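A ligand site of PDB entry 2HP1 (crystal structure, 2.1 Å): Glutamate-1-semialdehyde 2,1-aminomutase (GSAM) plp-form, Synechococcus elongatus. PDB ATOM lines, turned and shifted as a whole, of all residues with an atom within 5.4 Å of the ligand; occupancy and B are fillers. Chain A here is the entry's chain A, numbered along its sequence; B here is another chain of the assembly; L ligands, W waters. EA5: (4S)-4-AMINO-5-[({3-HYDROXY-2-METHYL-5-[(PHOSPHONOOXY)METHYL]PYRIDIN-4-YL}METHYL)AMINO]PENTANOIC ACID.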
ATOM      1  N   SER A  28     -23.021 -29.708   0.725  1.00  0.00           N
ATOM      2  CA  SER A  28     -23.129 -28.261   0.820  1.00  0.00           C
ATOM      3  C   SER A  28     -22.350 -27.628  -0.335  1.00  0.00           C
ATOM      4  O   SER A  28     -21.170 -27.936  -0.536  1.00  0.00           O
ATOM      5  CB  SER A  28     -22.600 -27.763   2.159  1.00  0.00           C
ATOM      6  OG  SER A  28     -22.829 -26.362   2.276  1.00  0.00           O
ATOM      7  N   VAL A  30     -20.870 -24.903  -0.792  1.00  0.00           N
ATOM      8  CA  VAL A  30     -19.637 -24.203  -0.478  1.00  0.00           C
ATOM      9  C   VAL A  30     -18.416 -25.098  -0.656  1.00  0.00           C
ATOM     10  O   VAL A  30     -17.293 -24.602  -0.768  1.00  0.00           O
ATOM     11  CB  VAL A  30     -19.676 -23.686   0.965  1.00  0.00           C
ATOM     12  CG1 VAL A  30     -19.467 -24.830   1.950  1.00  0.00           C
ATOM     13  CG2 VAL A  30     -18.631 -22.613   1.143  1.00  0.00           C
ATOM     14  N   ARG A  31     -18.634 -26.412  -0.698  1.00  0.00           N
ATOM     15  CA  ARG A  31     -17.545 -27.373  -0.855  1.00  0.00           C
ATOM     16  C   ARG A  31     -17.248 -27.738  -2.311  1.00  0.00           C
ATOM     17  O   ARG A  31     -16.330 -28.512  -2.582  1.00  0.00           O
ATOM     18  CB  ARG A  31     -17.877 -28.658  -0.076  1.00  0.00           C
ATOM     19  CG  ARG A  31     -18.217 -28.419   1.380  1.00  0.00           C
ATOM     20  CD  ARG A  31     -18.849 -29.661   2.013  1.00  0.00           C
ATOM     21  NE  ARG A  31     -19.384 -29.388   3.345  1.00  0.00           N
ATOM     22  CZ  ARG A  31     -20.044 -30.259   4.087  1.00  0.00           C
ATOM     23  NH1 ARG A  31     -20.261 -31.490   3.644  1.00  0.00           N
ATOM     24  NH2 ARG A  31     -20.523 -29.903   5.275  1.00  0.00           N
ATOM     25  N   TRP A  66     -15.351 -24.773   8.574  1.00  0.00           N
ATOM     26  CA  TRP A  66     -16.062 -23.499   8.406  1.00  0.00           C
ATOM     27  C   TRP A  66     -16.445 -22.736   9.662  1.00  0.00           C
ATOM     28  O   TRP A  66     -17.508 -22.114   9.722  1.00  0.00           O
ATOM     29  CB  TRP A  66     -17.297 -23.703   7.513  1.00  0.00           C
ATOM     30  CG  TRP A  66     -16.965 -24.390   6.227  1.00  0.00           C
ATOM     31  CD1 TRP A  66     -16.822 -25.738   6.022  1.00  0.00           C
ATOM     32  CD2 TRP A  66     -16.632 -23.768   4.979  1.00  0.00           C
ATOM     33  NE1 TRP A  66     -16.419 -25.988   4.737  1.00  0.00           N
ATOM     34  CE2 TRP A  66     -16.293 -24.791   4.076  1.00  0.00           C
ATOM     35  CE3 TRP A  66     -16.577 -22.428   4.549  1.00  0.00           C
ATOM     36  CZ2 TRP A  66     -15.912 -24.534   2.754  1.00  0.00           C
ATOM     37  CZ3 TRP A  66     -16.193 -22.168   3.236  1.00  0.00           C
ATOM     38  CH2 TRP A  66     -15.869 -23.220   2.358  1.00  0.00           C
ATOM     39  N   SER A 121     -29.059 -25.698  13.752  1.00  0.00           N
ATOM     40  CA  SER A 121     -28.131 -25.095  12.799  1.00  0.00           C
ATOM     41  C   SER A 121     -28.331 -23.578  12.759  1.00  0.00           C
ATOM     42  O   SER A 121     -29.291 -23.068  13.328  1.00  0.00           O
ATOM     43  CB  SER A 121     -28.351 -25.657  11.401  1.00  0.00           C
ATOM     44  OG  SER A 121     -29.610 -25.253  10.892  1.00  0.00           O
ATOM     45  N   GLY A 122     -27.426 -22.880  12.091  1.00  0.00           N
ATOM     46  CA  GLY A 122     -27.544 -21.441  11.961  1.00  0.00           C
ATOM     47  C   GLY A 122     -28.714 -21.099  11.057  1.00  0.00           C
ATOM     48  O   GLY A 122     -29.375 -20.065  11.236  1.00  0.00           O
ATOM     49  N   THR A 123     -28.995 -21.962  10.085  1.00  0.00           N
ATOM     50  CA  THR A 123     -30.117 -21.750   9.174  1.00  0.00           C
ATOM     51  C   THR A 123     -31.429 -21.732   9.942  1.00  0.00           C
ATOM     52  O   THR A 123     -32.293 -20.896   9.680  1.00  0.00           O
ATOM     53  CB  THR A 123     -30.158 -22.831   8.084  1.00  0.00           C
ATOM     54  OG1 THR A 123     -29.124 -22.569   7.119  1.00  0.00           O
ATOM     55  CG2 THR A 123     -31.521 -22.837   7.367  1.00  0.00           C
ATOM     56  N   GLU A 124     -31.573 -22.657  10.895  1.00  0.00           N
ATOM     57  CA  GLU A 124     -32.793 -22.726  11.694  1.00  0.00           C
ATOM     58  C   GLU A 124     -32.880 -21.535  12.636  1.00  0.00           C
ATOM     59  O   GLU A 124     -33.953 -20.956  12.824  1.00  0.00           O
ATOM     60  CB  GLU A 124     -32.840 -24.038  12.509  1.00  0.00           C
ATOM     61  CG  GLU A 124     -33.119 -25.290  11.685  1.00  0.00           C
ATOM     62  CD  GLU A 124     -33.364 -26.529  12.553  1.00  0.00           C
ATOM     63  OE1 GLU A 124     -33.046 -26.494  13.759  1.00  0.00           O
ATOM     64  OE2 GLU A 124     -33.871 -27.541  12.023  1.00  0.00           O
ATOM     65  N   CYS A 126     -31.598 -18.515  12.248  1.00  0.00           N
ATOM     66  CA  CYS A 126     -31.935 -17.303  11.504  1.00  0.00           C
ATOM     67  C   CYS A 126     -33.395 -17.310  11.050  1.00  0.00           C
ATOM     68  O   CYS A 126     -34.091 -16.296  11.149  1.00  0.00           O
ATOM     69  CB  CYS A 126     -31.000 -17.152  10.310  1.00  0.00           C
ATOM     70  SG  CYS A 126     -29.253 -16.834  10.755  1.00  0.00           S
ATOM     71  N   TYR A 149     -24.965 -13.546   4.520  1.00  0.00           N
ATOM     72  CA  TYR A 149     -25.635 -14.848   4.402  1.00  0.00           C
ATOM     73  C   TYR A 149     -26.230 -15.225   5.745  1.00  0.00           C
ATOM     74  O   TYR A 149     -25.550 -15.160   6.767  1.00  0.00           O
ATOM     75  CB  TYR A 149     -24.641 -15.918   3.949  1.00  0.00           C
ATOM     76  CG  TYR A 149     -25.237 -17.308   3.813  1.00  0.00           C
ATOM     77  CD1 TYR A 149     -26.199 -17.590   2.845  1.00  0.00           C
ATOM     78  CD2 TYR A 149     -24.849 -18.345   4.661  1.00  0.00           C
ATOM     79  CE1 TYR A 149     -26.767 -18.860   2.727  1.00  0.00           C
ATOM     80  CE2 TYR A 149     -25.410 -19.626   4.556  1.00  0.00           C
ATOM     81  CZ  TYR A 149     -26.368 -19.863   3.582  1.00  0.00           C
ATOM     82  OH  TYR A 149     -26.928 -21.123   3.470  1.00  0.00           O
ATOM     83  N   HIS A 150     -27.495 -15.604   5.756  1.00  0.00           N
ATOM     84  CA  HIS A 150     -28.165 -15.988   7.005  1.00  0.00           C
ATOM     85  C   HIS A 150     -28.911 -17.308   6.841  1.00  0.00           C
ATOM     86  O   HIS A 150     -30.066 -17.446   7.277  1.00  0.00           O
ATOM     87  CB  HIS A 150     -29.124 -14.874   7.433  1.00  0.00           C
ATOM     88  CG  HIS A 150     -28.489 -13.528   7.526  1.00  0.00           C
ATOM     89  ND1 HIS A 150     -27.443 -13.261   8.384  1.00  0.00           N
ATOM     90  CD2 HIS A 150     -28.751 -12.369   6.883  1.00  0.00           C
ATOM     91  CE1 HIS A 150     -27.089 -11.997   8.254  1.00  0.00           C
ATOM     92  NE2 HIS A 150     -27.870 -11.429   7.357  1.00  0.00           N
ATOM     93  N   GLY A 151     -28.258 -18.284   6.226  1.00  0.00           N
ATOM     94  CA  GLY A 151     -28.889 -19.563   6.023  1.00  0.00           C
ATOM     95  C   GLY A 151     -29.743 -19.497   4.773  1.00  0.00           C
ATOM     96  O   GLY A 151     -29.844 -18.444   4.146  1.00  0.00           O
ATOM     97  N   SER A 162     -21.671 -16.118   0.546  1.00  0.00           N
ATOM     98  CA  SER A 162     -21.339 -17.532   0.663  1.00  0.00           C
ATOM     99  C   SER A 162     -21.411 -18.203  -0.715  1.00  0.00           C
ATOM    100  O   SER A 162     -21.090 -17.592  -1.724  1.00  0.00           O
ATOM    101  CB  SER A 162     -22.293 -18.220   1.641  1.00  0.00           C
ATOM    102  OG  SER A 162     -21.922 -19.573   1.848  1.00  0.00           O
ATOM    103  N   GLU A 211     -24.466  -9.441   9.679  1.00  0.00           N
ATOM    104  CA  GLU A 211     -23.299 -10.066  10.268  1.00  0.00           C
ATOM    105  C   GLU A 211     -22.564  -8.815  10.777  1.00  0.00           C
ATOM    106  O   GLU A 211     -22.143  -7.992   9.975  1.00  0.00           O
ATOM    107  CB  GLU A 211     -22.461 -10.764   9.194  1.00  0.00           C
ATOM    108  CG  GLU A 211     -23.163 -11.921   8.489  1.00  0.00           C
ATOM    109  CD  GLU A 211     -22.326 -12.516   7.371  1.00  0.00           C
ATOM    110  OE1 GLU A 211     -21.138 -12.802   7.590  1.00  0.00           O
ATOM    111  OE2 GLU A 211     -22.870 -12.725   6.263  1.00  0.00           O
ATOM    112  N   ASN A 216     -19.042 -13.738   4.912  1.00  0.00           N
ATOM    113  CA  ASN A 216     -19.615 -14.380   3.733  1.00  0.00           C
ATOM    114  C   ASN A 216     -19.520 -13.684   2.397  1.00  0.00           C
ATOM    115  O   ASN A 216     -20.133 -14.105   1.413  1.00  0.00           O
ATOM    116  CB  ASN A 216     -21.070 -14.761   4.028  1.00  0.00           C
ATOM    117  CG  ASN A 216     -21.172 -15.939   4.972  1.00  0.00           C
ATOM    118  OD1 ASN A 216     -20.743 -17.048   4.639  1.00  0.00           O
ATOM    119  ND2 ASN A 216     -21.718 -15.710   6.157  1.00  0.00           N
ATOM    120  N   ASP A 244     -26.384 -11.461  13.389  1.00  0.00           N
ATOM    121  CA  ASP A 244     -26.208 -12.858  13.024  1.00  0.00           C
ATOM    122  C   ASP A 244     -24.764 -13.159  13.373  1.00  0.00           C
ATOM    123  O   ASP A 244     -23.855 -12.849  12.587  1.00  0.00           O
ATOM    124  CB  ASP A 244     -26.424 -13.069  11.533  1.00  0.00           C
ATOM    125  CG  ASP A 244     -26.199 -14.511  11.133  1.00  0.00           C
ATOM    126  OD1 ASP A 244     -25.678 -15.293  11.964  1.00  0.00           O
ATOM    127  OD2 ASP A 244     -26.534 -14.892   9.990  1.00  0.00           O
ATOM    128  N   VAL A 246     -23.618 -16.204  13.883  1.00  0.00           N
ATOM    129  CA  VAL A 246     -23.454 -17.627  13.651  1.00  0.00           C
ATOM    130  C   VAL A 246     -21.975 -17.911  13.356  1.00  0.00           C
ATOM    131  O   VAL A 246     -21.443 -18.932  13.776  1.00  0.00           O
ATOM    132  CB  VAL A 246     -24.299 -18.091  12.450  1.00  0.00           C
ATOM    133  CG1 VAL A 246     -23.825 -19.457  11.955  1.00  0.00           C
ATOM    134  CG2 VAL A 246     -25.769 -18.178  12.863  1.00  0.00           C
ATOM    135  N   MET A 247     -21.322 -16.985  12.664  1.00  0.00           N
ATOM    136  CA  MET A 247     -19.911 -17.140  12.327  1.00  0.00           C
ATOM    137  C   MET A 247     -18.997 -16.362  13.283  1.00  0.00           C
ATOM    138  O   MET A 247     -17.951 -16.860  13.695  1.00  0.00           O
ATOM    139  CB  MET A 247     -19.647 -16.666  10.886  1.00  0.00           C
ATOM    140  CG  MET A 247     -18.222 -16.945  10.418  1.00  0.00           C
ATOM    141  SD  MET A 247     -17.870 -16.325   8.769  1.00  0.00           S
ATOM    142  CE  MET A 247     -18.699 -17.545   7.752  1.00  0.00           C
ATOM    143  N   LYS A 272     -22.461 -22.890  14.480  1.00  0.00           N
ATOM    144  CA  LYS A 272     -21.069 -23.330  14.351  1.00  0.00           C
ATOM    145  C   LYS A 272     -20.385 -23.647  15.683  1.00  0.00           C
ATOM    146  O   LYS A 272     -20.585 -24.714  16.249  1.00  0.00           O
ATOM    147  CB  LYS A 272     -20.265 -22.263  13.609  1.00  0.00           C
ATOM    148  CG  LYS A 272     -20.701 -22.022  12.176  1.00  0.00           C
ATOM    149  CD  LYS A 272     -20.065 -20.755  11.644  1.00  0.00           C
ATOM    150  CE  LYS A 272     -20.404 -20.564  10.195  1.00  0.00           C
ATOM    151  NZ  LYS A 272     -19.983 -21.773   9.457  1.00  0.00           N
ATOM    152  N   GLU A 405     -15.128 -16.205   1.206  1.00  0.00           N
ATOM    153  CA  GLU A 405     -15.228 -16.843   2.503  1.00  0.00           C
ATOM    154  C   GLU A 405     -14.073 -16.403   3.379  1.00  0.00           C
ATOM    155  O   GLU A 405     -12.927 -16.391   2.932  1.00  0.00           O
ATOM    156  CB  GLU A 405     -15.188 -18.367   2.356  1.00  0.00           C
ATOM    157  CG  GLU A 405     -16.546 -19.046   2.440  1.00  0.00           C
ATOM    158  CD  GLU A 405     -17.231 -18.844   3.790  1.00  0.00           C
ATOM    159  OE1 GLU A 405     -16.568 -18.987   4.851  1.00  0.00           O
ATOM    160  OE2 GLU A 405     -18.444 -18.548   3.785  1.00  0.00           O
ATOM    161  N   PHE A 408     -10.194 -19.001   8.827  1.00  0.00           N
ATOM    162  CA  PHE A 408     -10.268 -19.224  10.256  1.00  0.00           C
ATOM    163  C   PHE A 408      -8.991 -19.859  10.824  1.00  0.00           C
ATOM    164  O   PHE A 408      -8.330 -20.657  10.148  1.00  0.00           O
ATOM    165  CB  PHE A 408     -11.463 -20.129  10.591  1.00  0.00           C
ATOM    166  CG  PHE A 408     -12.779 -19.611  10.096  1.00  0.00           C
ATOM    167  CD1 PHE A 408     -13.457 -20.264   9.077  1.00  0.00           C
ATOM    168  CD2 PHE A 408     -13.341 -18.456  10.645  1.00  0.00           C
ATOM    169  CE1 PHE A 408     -14.689 -19.789   8.613  1.00  0.00           C
ATOM    170  CE2 PHE A 408     -14.566 -17.970  10.186  1.00  0.00           C
ATOM    171  CZ  PHE A 408     -15.243 -18.639   9.161  1.00  0.00           C
ATOM    172  N   GLU B 124     -35.135 -28.599   7.837  1.00  0.00           N
ATOM    173  CA  GLU B 124     -34.275 -28.132   6.741  1.00  0.00           C
ATOM    174  C   GLU B 124     -34.664 -28.880   5.481  1.00  0.00           C
ATOM    175  O   GLU B 124     -34.728 -28.304   4.401  1.00  0.00           O
ATOM    176  CB  GLU B 124     -32.798 -28.372   7.048  1.00  0.00           C
ATOM    177  CG  GLU B 124     -32.259 -27.576   8.221  1.00  0.00           C
ATOM    178  CD  GLU B 124     -30.752 -27.607   8.307  1.00  0.00           C
ATOM    179  OE1 GLU B 124     -30.141 -28.526   7.732  1.00  0.00           O
ATOM    180  OE2 GLU B 124     -30.175 -26.718   8.964  1.00  0.00           O
ATOM    181  N   TYR B 300     -30.615 -22.595  -4.213  1.00  0.00           N
ATOM    182  CA  TYR B 300     -29.665 -22.645  -3.122  1.00  0.00           C
ATOM    183  C   TYR B 300     -30.183 -23.247  -1.842  1.00  0.00           C
ATOM    184  O   TYR B 300     -31.314 -23.018  -1.422  1.00  0.00           O
ATOM    185  CB  TYR B 300     -29.115 -21.252  -2.808  1.00  0.00           C
ATOM    186  CG  TYR B 300     -27.774 -21.316  -2.105  1.00  0.00           C
ATOM    187  CD1 TYR B 300     -26.621 -21.644  -2.796  1.00  0.00           C
ATOM    188  CD2 TYR B 300     -27.668 -21.066  -0.733  1.00  0.00           C
ATOM    189  CE1 TYR B 300     -25.388 -21.716  -2.155  1.00  0.00           C
ATOM    190  CE2 TYR B 300     -26.441 -21.131  -0.081  1.00  0.00           C
ATOM    191  CZ  TYR B 300     -25.306 -21.463  -0.799  1.00  0.00           C
ATOM    192  OH  TYR B 300     -24.073 -21.549  -0.185  1.00  0.00           O
ATOM    193  N   ALA B 302     -27.789 -24.867   1.684  1.00  0.00           N
ATOM    194  CA  ALA B 302     -26.479 -25.260   2.174  1.00  0.00           C
ATOM    195  C   ALA B 302     -26.579 -25.648   3.643  1.00  0.00           C
ATOM    196  O   ALA B 302     -27.653 -25.591   4.232  1.00  0.00           O
ATOM    197  CB  ALA B 302     -25.489 -24.107   2.003  1.00  0.00           C
ATOM    198  N   GLY B 303     -25.444 -26.036   4.221  1.00  0.00           N
ATOM    199  CA  GLY B 303     -25.432 -26.437   5.614  1.00  0.00           C
ATOM    200  C   GLY B 303     -24.041 -26.790   6.075  1.00  0.00           C
ATOM    201  O   GLY B 303     -23.420 -27.724   5.556  1.00  0.00           O
ATOM    202  N   THR B 304     -23.549 -26.028   7.054  1.00  0.00           N
ATOM    203  CA  THR B 304     -22.222 -26.240   7.622  1.00  0.00           C
ATOM    204  C   THR B 304     -22.003 -27.652   8.140  1.00  0.00           C
ATOM    205  O   THR B 304     -21.010 -28.289   7.799  1.00  0.00           O
ATOM    206  CB  THR B 304     -21.950 -25.282   8.797  1.00  0.00           C
ATOM    207  OG1 THR B 304     -22.188 -23.938   8.373  1.00  0.00           O
ATOM    208  CG2 THR B 304     -20.501 -25.406   9.252  1.00  0.00           C
ATOM    209  N   LEU B 305     -22.926 -28.145   8.967  1.00  0.00           N
ATOM    210  CA  LEU B 305     -22.766 -29.490   9.527  1.00  0.00           C
ATOM    211  C   LEU B 305     -23.322 -30.608   8.662  1.00  0.00           C
ATOM    212  O   LEU B 305     -23.236 -31.780   9.014  1.00  0.00           O
ATOM    213  CB  LEU B 305     -23.402 -29.543  10.921  1.00  0.00           C
ATOM    214  CG  LEU B 305     -22.516 -29.182  12.110  1.00  0.00           C
ATOM    215  CD1 LEU B 305     -21.499 -30.297  12.334  1.00  0.00           C
ATOM    216  CD2 LEU B 305     -21.808 -27.838  11.859  1.00  0.00           C
HETATM  217  P   EA5 L   1     -25.706 -23.165   9.149  1.00  0.00           P
HETATM  218  OP1 EA5 L   1     -25.443 -23.778  10.473  1.00  0.00           O
HETATM  219  OP2 EA5 L   1     -27.053 -23.660   8.520  1.00  0.00           O
HETATM  220  OP3 EA5 L   1     -24.904 -23.481   7.974  1.00  0.00           O
HETATM  221  OP4 EA5 L   1     -25.755 -21.584   9.325  1.00  0.00           O
HETATM  222  C5A EA5 L   1     -26.032 -20.676   8.219  1.00  0.00           C
HETATM  223  C5  EA5 L   1     -25.305 -19.349   8.474  1.00  0.00           C
HETATM  224  C6  EA5 L   1     -26.033 -18.292   8.944  1.00  0.00           C
HETATM  225  N1  EA5 L   1     -25.403 -17.098   9.176  1.00  0.00           N
HETATM  226  C2  EA5 L   1     -24.043 -16.920   8.946  1.00  0.00           C
HETATM  227  C2A EA5 L   1     -23.419 -15.535   9.227  1.00  0.00           C
HETATM  228  C3  EA5 L   1     -23.281 -17.976   8.464  1.00  0.00           C
HETATM  229  O3  EA5 L   1     -21.903 -17.825   8.226  1.00  0.00           O
HETATM  230  C4  EA5 L   1     -23.921 -19.206   8.225  1.00  0.00           C
HETATM  231  C4A EA5 L   1     -23.142 -20.397   7.694  1.00  0.00           C
HETATM  232  N4A EA5 L   1     -21.809 -20.348   7.426  1.00  0.00           N
HETATM  233  N4  EA5 L   1     -18.772 -20.892   6.404  1.00  0.00           N
HETATM  234  CA  EA5 L   1     -20.109 -21.212   5.836  1.00  0.00           C
HETATM  235  C   EA5 L   1     -21.153 -21.554   6.929  1.00  0.00           C
HETATM  236  CB  EA5 L   1     -19.981 -22.325   4.744  1.00  0.00           C
HETATM  237  CG  EA5 L   1     -20.397 -23.774   5.109  1.00  0.00           C
HETATM  238  CD  EA5 L   1     -21.743 -24.221   4.529  1.00  0.00           C
HETATM  239  OE1 EA5 L   1     -22.621 -23.364   4.243  1.00  0.00           O
HETATM  240  OE2 EA5 L   1     -21.933 -25.431   4.378  1.00  0.00           O
HETATM  241  O   HOH W   1     -25.279 -22.945   5.214  1.00  0.00           O
HETATM  242  O   HOH W   2     -21.772 -14.428  12.005  1.00  0.00           O
HETATM  243  O   HOH W   3     -23.688 -21.325   2.479  1.00  0.00           O
HETATM  244  O   HOH W   4     -27.737 -26.232   7.982  1.00  0.00           O
HETATM  245  O   HOH W   5     -23.444 -23.969  12.312  1.00  0.00           O
HETATM  246  O   HOH W   6     -25.307 -26.597   9.778  1.00  0.00           O
HETATM  247  O   HOH W   7     -19.555 -26.967   4.699  1.00  0.00           O
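An oxygen (OE2) of the ligand sits at hydrogen-bond distance from the side-chain hydroxyl of Ser 28 (2.5 Å).
OD2 of Asp 244 is in hydrogen-bond range of N1 of the ligand (2.6 Å).
The backbone NH (N) of Gly 122 is in hydrogen-bond range of an oxygen (OP1) of the ligand (2.7 Å).
The backbone NH (N) of Thr 123 sits at hydrogen-bond distance from an oxygen (OP2) of the ligand, at 3.0 Å.
The side-chain hydroxyl (OG1) of Thr 123 sits at hydrogen-bond distance from an oxygen (OP2) of the ligand (2.7 Å).
The backbone NH (N) of Thr 304 of chain B sits at hydrogen-bond distance from an oxygen (OP3) of the ligand, at 3.0 Å.
An oxygen (OP3) of the ligand sits at hydrogen-bond distance from the side-chain hydroxyl of Thr 304 of chain B (2.8 Å).
A nitrogen (N4A) of the ligand lies close to the side-chain amino group of Lys 272 (3.1 Å).
O3 of the ligand is in hydrogen-bond range of ND2 of Asn 216, 3.0 Å away.
O of Gly 303 of chain B sits close to OE2 of the ligand, 3.0 Å away.
OE1 of Glu 405 lies within salt-bridge range of N4 of the ligand, at 3.3 Å.
The backbone NH (N) of Val 246 lies within hydrogen-bond range of the side-chain carboxylate (OD1) of Asp 244 (3.0 Å).
OD2 of Asp 244 lies within hydrogen-bond range of ND1 of His 150 (2.5 Å).
The backbone carbonyl oxygen (O) of Gly 122 is in hydrogen-bond range of the side-chain sulfur (SG) of Cys 126 (3.3 Å).
The backbone NH (N) of Thr 123 sits close to the side-chain hydroxyl (OG) of Ser 121, at 3.4 Å.
The side-chain amino group (NZ) of Lys 272 lies within hydrogen-bond range of the side-chain hydroxyl (OG1) of Thr 304 of chain B (3.3 Å).
The backbone NH (N) of Tyr 149 sits at hydrogen-bond distance from the side-chain carboxylate (OE2) of Glu 211 (2.8 Å).
OG of Ser 121 sits at hydrogen-bond distance from N of Glu 124 of chain A, 3.3 Å away.
SG of Cys 126 lies close to O of His 150, at 3.6 Å.
O of Tyr 149 lies close to N1 of the ligand (3.1 Å).
Merely in contact with the ligand: Val 30 (3.5 Å), Trp 66 (3.3 Å), Ser 121 (3.6 Å), Cys 126 (3.97 Å), His 150 (3.7 Å), Gly 151 (3.5 Å), Glu 211 (3.7 Å), Val 246 (3.6 Å), Met 247 (3.3 Å) and Ala 302 of chain B (3.7 Å).
Hydrophobic or aromatic side chains that line the ligand: Val 30, Trp 66, Tyr 149, Val 246, Met 247 and Ala 302 of chain B.
The nearest printed residue that does not touch the ligand is Glu 124 of chain B (4.4 Å).
Water W4 bridges the side-chain carboxylate of Glu 124 of chain B (2.7 Å) and an oxygen (OP2) of the ligand (2.7 Å).
Water W5 lies within hydrogen-bond range of N of Lys 272 (2.6 Å) and OP1 of the ligand (2.7 Å).
Water W1 lies within hydrogen-bond range of OP3 of the ligand (2.8 Å), OH of Tyr 149 (3.0 Å) and N of Gly 303 of chain B (3.3 Å).
Water W7 lies within hydrogen-bond range of the guanidinium group of Arg 31, an oxygen (OE2) of the ligand and the indole nitrogen of Trp 66.
Water W3 lies within hydrogen-bond range of OG of Ser 162 (2.6 Å), OH of Tyr 300 of chain B (2.7 Å), OE1 of the ligand (2.9 Å) and OH of Tyr 149 (3.4 Å).
Water W6 lies within hydrogen-bond range of OP1 of the ligand (2.9 Å), N of Leu 305 of chain B (3.0 Å) and N of Thr 304 of chain B (3.3 Å).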
